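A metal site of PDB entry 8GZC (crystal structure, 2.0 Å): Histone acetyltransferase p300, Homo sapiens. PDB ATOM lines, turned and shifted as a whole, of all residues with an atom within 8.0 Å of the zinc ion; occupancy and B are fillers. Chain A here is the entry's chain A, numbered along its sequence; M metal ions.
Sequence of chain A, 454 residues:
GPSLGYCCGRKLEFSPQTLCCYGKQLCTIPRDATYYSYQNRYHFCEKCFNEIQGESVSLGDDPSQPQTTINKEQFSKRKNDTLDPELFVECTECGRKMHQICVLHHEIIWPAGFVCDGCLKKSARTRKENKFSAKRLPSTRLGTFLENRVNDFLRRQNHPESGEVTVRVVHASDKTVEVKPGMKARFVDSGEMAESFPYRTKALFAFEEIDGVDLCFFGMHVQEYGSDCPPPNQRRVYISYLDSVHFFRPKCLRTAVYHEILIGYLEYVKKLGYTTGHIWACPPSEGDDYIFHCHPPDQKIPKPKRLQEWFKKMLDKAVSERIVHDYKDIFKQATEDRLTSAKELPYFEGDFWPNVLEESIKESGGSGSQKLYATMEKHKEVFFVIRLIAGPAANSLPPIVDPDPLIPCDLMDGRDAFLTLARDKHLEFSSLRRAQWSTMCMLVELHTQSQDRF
The zinc ion is bound by the side-chain sulfur (SG) of Cys 21 (2.3 Å), the side-chain sulfur (SG) of Cys 48 (2.3 Å), the side-chain sulfur (SG) of Cys 27 (2.3 Å) and the side-chain sulfur (SG) of Cys 45 (2.3 Å). The zinc ion has four donor atoms within binding distance.
The backbone carbonyl oxygen (O) of His 43 lies close to the backbone carbonyl oxygen (O) of Cys 21 (2.6 Å). SG of Cys 45 sits close to N of Lys 47, 3.7 Å away. The side-chain sulfur (SG) of Cys 21 sits close to the backbone NH (N) of Gly 23.
Of the 19 residues printed, 4 come within 4 Å of the zinc ion. The nearest printed residue that does not touch the zinc ion is Lys 24 (4.6 Å).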
ATOM      1  N   LEU A  19     -11.173   5.036 -22.597  1.00  0.00           N
ATOM      2  CA  LEU A  19     -11.129   3.883 -23.488  1.00  0.00           C
ATOM      3  C   LEU A  19     -12.239   2.902 -23.103  1.00  0.00           C
ATOM      4  O   LEU A  19     -13.005   3.140 -22.170  1.00  0.00           O
ATOM      5  CB  LEU A  19      -9.755   3.218 -23.426  1.00  0.00           C
ATOM      6  CG  LEU A  19      -8.630   4.008 -22.742  1.00  0.00           C
ATOM      7  CD1 LEU A  19      -7.669   3.079 -22.017  1.00  0.00           C
ATOM      8  CD2 LEU A  19      -7.889   4.874 -23.751  1.00  0.00           C
ATOM      9  N   CYS A  20     -12.328   1.805 -23.848  1.00  0.00           N
ATOM     10  CA  CYS A  20     -13.275   0.738 -23.544  1.00  0.00           C
ATOM     11  C   CYS A  20     -12.530  -0.460 -22.949  1.00  0.00           C
ATOM     12  O   CYS A  20     -11.322  -0.619 -23.132  1.00  0.00           O
ATOM     13  CB  CYS A  20     -14.040   0.307 -24.794  1.00  0.00           C
ATOM     14  SG  CYS A  20     -13.080   0.403 -26.326  1.00  0.00           S
ATOM     15  N   CYS A  21     -13.276  -1.299 -22.231  1.00  0.00           N
ATOM     16  CA  CYS A  21     -12.656  -2.385 -21.476  1.00  0.00           C
ATOM     17  C   CYS A  21     -12.828  -3.756 -22.117  1.00  0.00           C
ATOM     18  O   CYS A  21     -12.262  -4.731 -21.612  1.00  0.00           O
ATOM     19  CB  CYS A  21     -13.212  -2.398 -20.052  1.00  0.00           C
ATOM     20  SG  CYS A  21     -14.326  -3.741 -19.708  1.00  0.00           S
ATOM     21  N   TYR A  22     -13.638  -3.881 -23.178  1.00  0.00           N
ATOM     22  CA  TYR A  22     -13.660  -5.041 -24.059  1.00  0.00           C
ATOM     23  C   TYR A  22     -14.177  -6.308 -23.382  1.00  0.00           C
ATOM     24  O   TYR A  22     -14.551  -7.267 -24.056  1.00  0.00           O
ATOM     25  CB  TYR A  22     -12.260  -5.324 -24.623  1.00  0.00           C
ATOM     26  CG  TYR A  22     -12.243  -6.385 -25.709  1.00  0.00           C
ATOM     27  CD1 TYR A  22     -12.637  -6.081 -27.005  1.00  0.00           C
ATOM     28  CD2 TYR A  22     -11.862  -7.699 -25.429  1.00  0.00           C
ATOM     29  CE1 TYR A  22     -12.646  -7.042 -28.000  1.00  0.00           C
ATOM     30  CE2 TYR A  22     -11.865  -8.672 -26.428  1.00  0.00           C
ATOM     31  CZ  TYR A  22     -12.263  -8.330 -27.702  1.00  0.00           C
ATOM     32  OH  TYR A  22     -12.267  -9.285 -28.704  1.00  0.00           O
ATOM     33  N   GLY A  23     -14.272  -6.280 -22.060  1.00  0.00           N
ATOM     34  CA  GLY A  23     -14.602  -7.474 -21.306  1.00  0.00           C
ATOM     35  C   GLY A  23     -15.953  -7.315 -20.647  1.00  0.00           C
ATOM     36  O   GLY A  23     -16.290  -8.023 -19.684  1.00  0.00           O
ATOM     37  N   LYS A  24     -16.707  -6.355 -21.152  1.00  0.00           N
ATOM     38  CA  LYS A  24     -18.061  -6.055 -20.722  1.00  0.00           C
ATOM     39  C   LYS A  24     -18.658  -5.100 -21.735  1.00  0.00           C
ATOM     40  O   LYS A  24     -17.982  -4.156 -22.159  1.00  0.00           O
ATOM     41  CB  LYS A  24     -18.086  -5.432 -19.316  1.00  0.00           C
ATOM     42  N   GLN A  25     -19.906  -5.338 -22.129  1.00  0.00           N
ATOM     43  CA  GLN A  25     -20.560  -4.457 -23.080  1.00  0.00           C
ATOM     44  C   GLN A  25     -20.685  -3.061 -22.489  1.00  0.00           C
ATOM     45  O   GLN A  25     -21.162  -2.881 -21.373  1.00  0.00           O
ATOM     46  CB  GLN A  25     -21.931  -5.002 -23.454  1.00  0.00           C
ATOM     47  N   LEU A  26     -20.207  -2.071 -23.252  1.00  0.00           N
ATOM     48  CA  LEU A  26     -20.348  -0.652 -22.896  1.00  0.00           C
ATOM     49  C   LEU A  26     -19.687  -0.306 -21.563  1.00  0.00           C
ATOM     50  O   LEU A  26     -20.194   0.510 -20.792  1.00  0.00           O
ATOM     51  CB  LEU A  26     -21.825  -0.243 -22.879  1.00  0.00           C
ATOM     52  CG  LEU A  26     -22.589  -0.371 -24.209  1.00  0.00           C
ATOM     53  CD1 LEU A  26     -24.072  -0.125 -23.983  1.00  0.00           C
ATOM     54  CD2 LEU A  26     -22.036   0.588 -25.240  1.00  0.00           C
ATOM     55  N   CYS A  27     -18.532  -0.920 -21.291  1.00  0.00           N
ATOM     56  CA  CYS A  27     -17.693  -0.539 -20.163  1.00  0.00           C
ATOM     57  C   CYS A  27     -16.580   0.380 -20.654  1.00  0.00           C
ATOM     58  O   CYS A  27     -16.168   0.314 -21.814  1.00  0.00           O
ATOM     59  CB  CYS A  27     -17.100  -1.756 -19.456  1.00  0.00           C
ATOM     60  SG  CYS A  27     -16.332  -1.427 -17.833  1.00  0.00           S
ATOM     61  N   THR A  28     -16.095   1.237 -19.754  1.00  0.00           N
ATOM     62  CA  THR A  28     -15.073   2.216 -20.125  1.00  0.00           C
ATOM     63  C   THR A  28     -14.012   2.308 -19.045  1.00  0.00           C
ATOM     64  O   THR A  28     -14.230   1.963 -17.880  1.00  0.00           O
ATOM     65  CB  THR A  28     -15.658   3.612 -20.377  1.00  0.00           C
ATOM     66  OG1 THR A  28     -16.367   4.062 -19.219  1.00  0.00           O
ATOM     67  CG2 THR A  28     -16.603   3.595 -21.580  1.00  0.00           C
ATOM     68  N   ILE A  29     -12.835   2.780 -19.458  1.00  0.00           N
ATOM     69  CA  ILE A  29     -11.705   3.078 -18.587  1.00  0.00           C
ATOM     70  C   ILE A  29     -11.472   4.585 -18.621  1.00  0.00           C
ATOM     71  O   ILE A  29     -11.095   5.124 -19.671  1.00  0.00           O
ATOM     72  CB  ILE A  29     -10.446   2.316 -19.030  1.00  0.00           C
ATOM     73  CG1 ILE A  29     -10.757   0.827 -19.163  1.00  0.00           C
ATOM     74  CG2 ILE A  29      -9.309   2.561 -18.044  1.00  0.00           C
ATOM     75  CD1 ILE A  29      -9.580  -0.016 -19.494  1.00  0.00           C
ATOM     76  N   HIS A  43      -8.006  -3.497 -24.291  1.00  0.00           N
ATOM     77  CA  HIS A  43      -7.838  -2.864 -22.992  1.00  0.00           C
ATOM     78  C   HIS A  43      -8.890  -3.400 -22.028  1.00  0.00           C
ATOM     79  O   HIS A  43     -10.010  -3.721 -22.428  1.00  0.00           O
ATOM     80  CB  HIS A  43      -7.960  -1.339 -23.115  1.00  0.00           C
ATOM     81  CG  HIS A  43      -7.198  -0.771 -24.280  1.00  0.00           C
ATOM     82  ND1 HIS A  43      -5.882  -0.392 -24.180  1.00  0.00           N
ATOM     83  CD2 HIS A  43      -7.564  -0.552 -25.562  1.00  0.00           C
ATOM     84  CE1 HIS A  43      -5.470   0.055 -25.350  1.00  0.00           C
ATOM     85  NE2 HIS A  43      -6.466  -0.025 -26.212  1.00  0.00           N
ATOM     86  N   PHE A  44      -8.496  -3.520 -20.758  1.00  0.00           N
ATOM     87  CA  PHE A  44      -9.376  -4.067 -19.728  1.00  0.00           C
ATOM     88  C   PHE A  44      -9.316  -3.202 -18.486  1.00  0.00           C
ATOM     89  O   PHE A  44      -8.219  -2.876 -18.003  1.00  0.00           O
ATOM     90  CB  PHE A  44      -8.967  -5.500 -19.350  1.00  0.00           C
ATOM     91  CG  PHE A  44      -9.372  -6.544 -20.352  1.00  0.00           C
ATOM     92  CD1 PHE A  44      -8.720  -6.642 -21.566  1.00  0.00           C
ATOM     93  CD2 PHE A  44     -10.401  -7.425 -20.068  1.00  0.00           C
ATOM     94  CE1 PHE A  44      -9.086  -7.602 -22.490  1.00  0.00           C
ATOM     95  CE2 PHE A  44     -10.772  -8.390 -20.984  1.00  0.00           C
ATOM     96  CZ  PHE A  44     -10.112  -8.477 -22.199  1.00  0.00           C
ATOM     97  N   CYS A  45     -10.473  -2.826 -17.958  1.00  0.00           N
ATOM     98  CA  CYS A  45     -10.512  -2.283 -16.613  1.00  0.00           C
ATOM     99  C   CYS A  45     -10.156  -3.381 -15.621  1.00  0.00           C
ATOM    100  O   CYS A  45     -10.317  -4.575 -15.899  1.00  0.00           O
ATOM    101  CB  CYS A  45     -11.878  -1.675 -16.308  1.00  0.00           C
ATOM    102  SG  CYS A  45     -13.119  -2.862 -15.775  1.00  0.00           S
ATOM    103  N   GLU A  46      -9.657  -2.980 -14.453  1.00  0.00           N
ATOM    104  CA  GLU A  46      -9.171  -3.954 -13.490  1.00  0.00           C
ATOM    105  C   GLU A  46     -10.259  -4.958 -13.107  1.00  0.00           C
ATOM    106  O   GLU A  46     -10.008  -6.155 -13.027  1.00  0.00           O
ATOM    107  CB  GLU A  46      -8.626  -3.247 -12.241  1.00  0.00           C
ATOM    108  CG  GLU A  46      -7.470  -3.995 -11.576  1.00  0.00           C
ATOM    109  CD  GLU A  46      -6.727  -3.132 -10.562  1.00  0.00           C
ATOM    110  OE1 GLU A  46      -7.106  -1.957 -10.399  1.00  0.00           O
ATOM    111  OE2 GLU A  46      -5.774  -3.628  -9.943  1.00  0.00           O
ATOM    112  N   LYS A  47     -11.488  -4.463 -12.902  1.00  0.00           N
ATOM    113  CA  LYS A  47     -12.587  -5.361 -12.550  1.00  0.00           C
ATOM    114  C   LYS A  47     -12.850  -6.380 -13.665  1.00  0.00           C
ATOM    115  O   LYS A  47     -12.957  -7.584 -13.400  1.00  0.00           O
ATOM    116  CB  LYS A  47     -13.849  -4.552 -12.265  1.00  0.00           C
ATOM    117  N   CYS A  48     -12.946  -5.908 -14.903  1.00  0.00           N
ATOM    118  CA  CYS A  48     -13.219  -6.828 -16.012  1.00  0.00           C
ATOM    119  C   CYS A  48     -12.065  -7.820 -16.201  1.00  0.00           C
ATOM    120  O   CYS A  48     -12.290  -8.938 -16.653  1.00  0.00           O
ATOM    121  CB  CYS A  48     -13.461  -6.031 -17.295  1.00  0.00           C
ATOM    122  SG  CYS A  48     -15.109  -5.266 -17.345  1.00  0.00           S
ATOM    123  N   PHE A  49     -10.844  -7.424 -15.839  1.00  0.00           N
ATOM    124  CA  PHE A  49      -9.703  -8.331 -15.926  1.00  0.00           C
ATOM    125  C   PHE A  49      -9.761  -9.401 -14.851  1.00  0.00           C
ATOM    126  O   PHE A  49      -9.613 -10.600 -15.138  1.00  0.00           O
ATOM    127  CB  PHE A  49      -8.402  -7.539 -15.830  1.00  0.00           C
ATOM    128  CG  PHE A  49      -7.245  -8.176 -16.543  1.00  0.00           C
ATOM    129  CD1 PHE A  49      -7.303  -8.421 -17.897  1.00  0.00           C
ATOM    130  CD2 PHE A  49      -6.093  -8.522 -15.844  1.00  0.00           C
ATOM    131  CE1 PHE A  49      -6.231  -9.008 -18.560  1.00  0.00           C
ATOM    132  CE2 PHE A  49      -5.025  -9.114 -16.499  1.00  0.00           C
ATOM    133  CZ  PHE A  49      -5.092  -9.354 -17.854  1.00  0.00           C
ATOM    134  N   GLU A  51     -12.237 -10.538 -13.212  1.00  0.00           N
ATOM    135  CA  GLU A  51     -13.390 -11.413 -13.355  1.00  0.00           C
ATOM    136  C   GLU A  51     -13.222 -12.430 -14.470  1.00  0.00           C
ATOM    137  O   GLU A  51     -14.099 -13.290 -14.642  1.00  0.00           O
ATOM    138  CB  GLU A  51     -14.654 -10.582 -13.590  1.00  0.00           C
ATOM    139  CG  GLU A  51     -15.291 -10.057 -12.300  1.00  0.00           C
ATOM    140  CD  GLU A  51     -15.683  -8.594 -12.395  1.00  0.00           C
ATOM    141  OE1 GLU A  51     -15.965  -8.118 -13.513  1.00  0.00           O
ATOM    142  OE2 GLU A  51     -15.732  -7.919 -11.342  1.00  0.00           O
HETATM  143 ZN    ZN M   1     -14.637  -3.001 -17.540  1.00  0.00          ZN
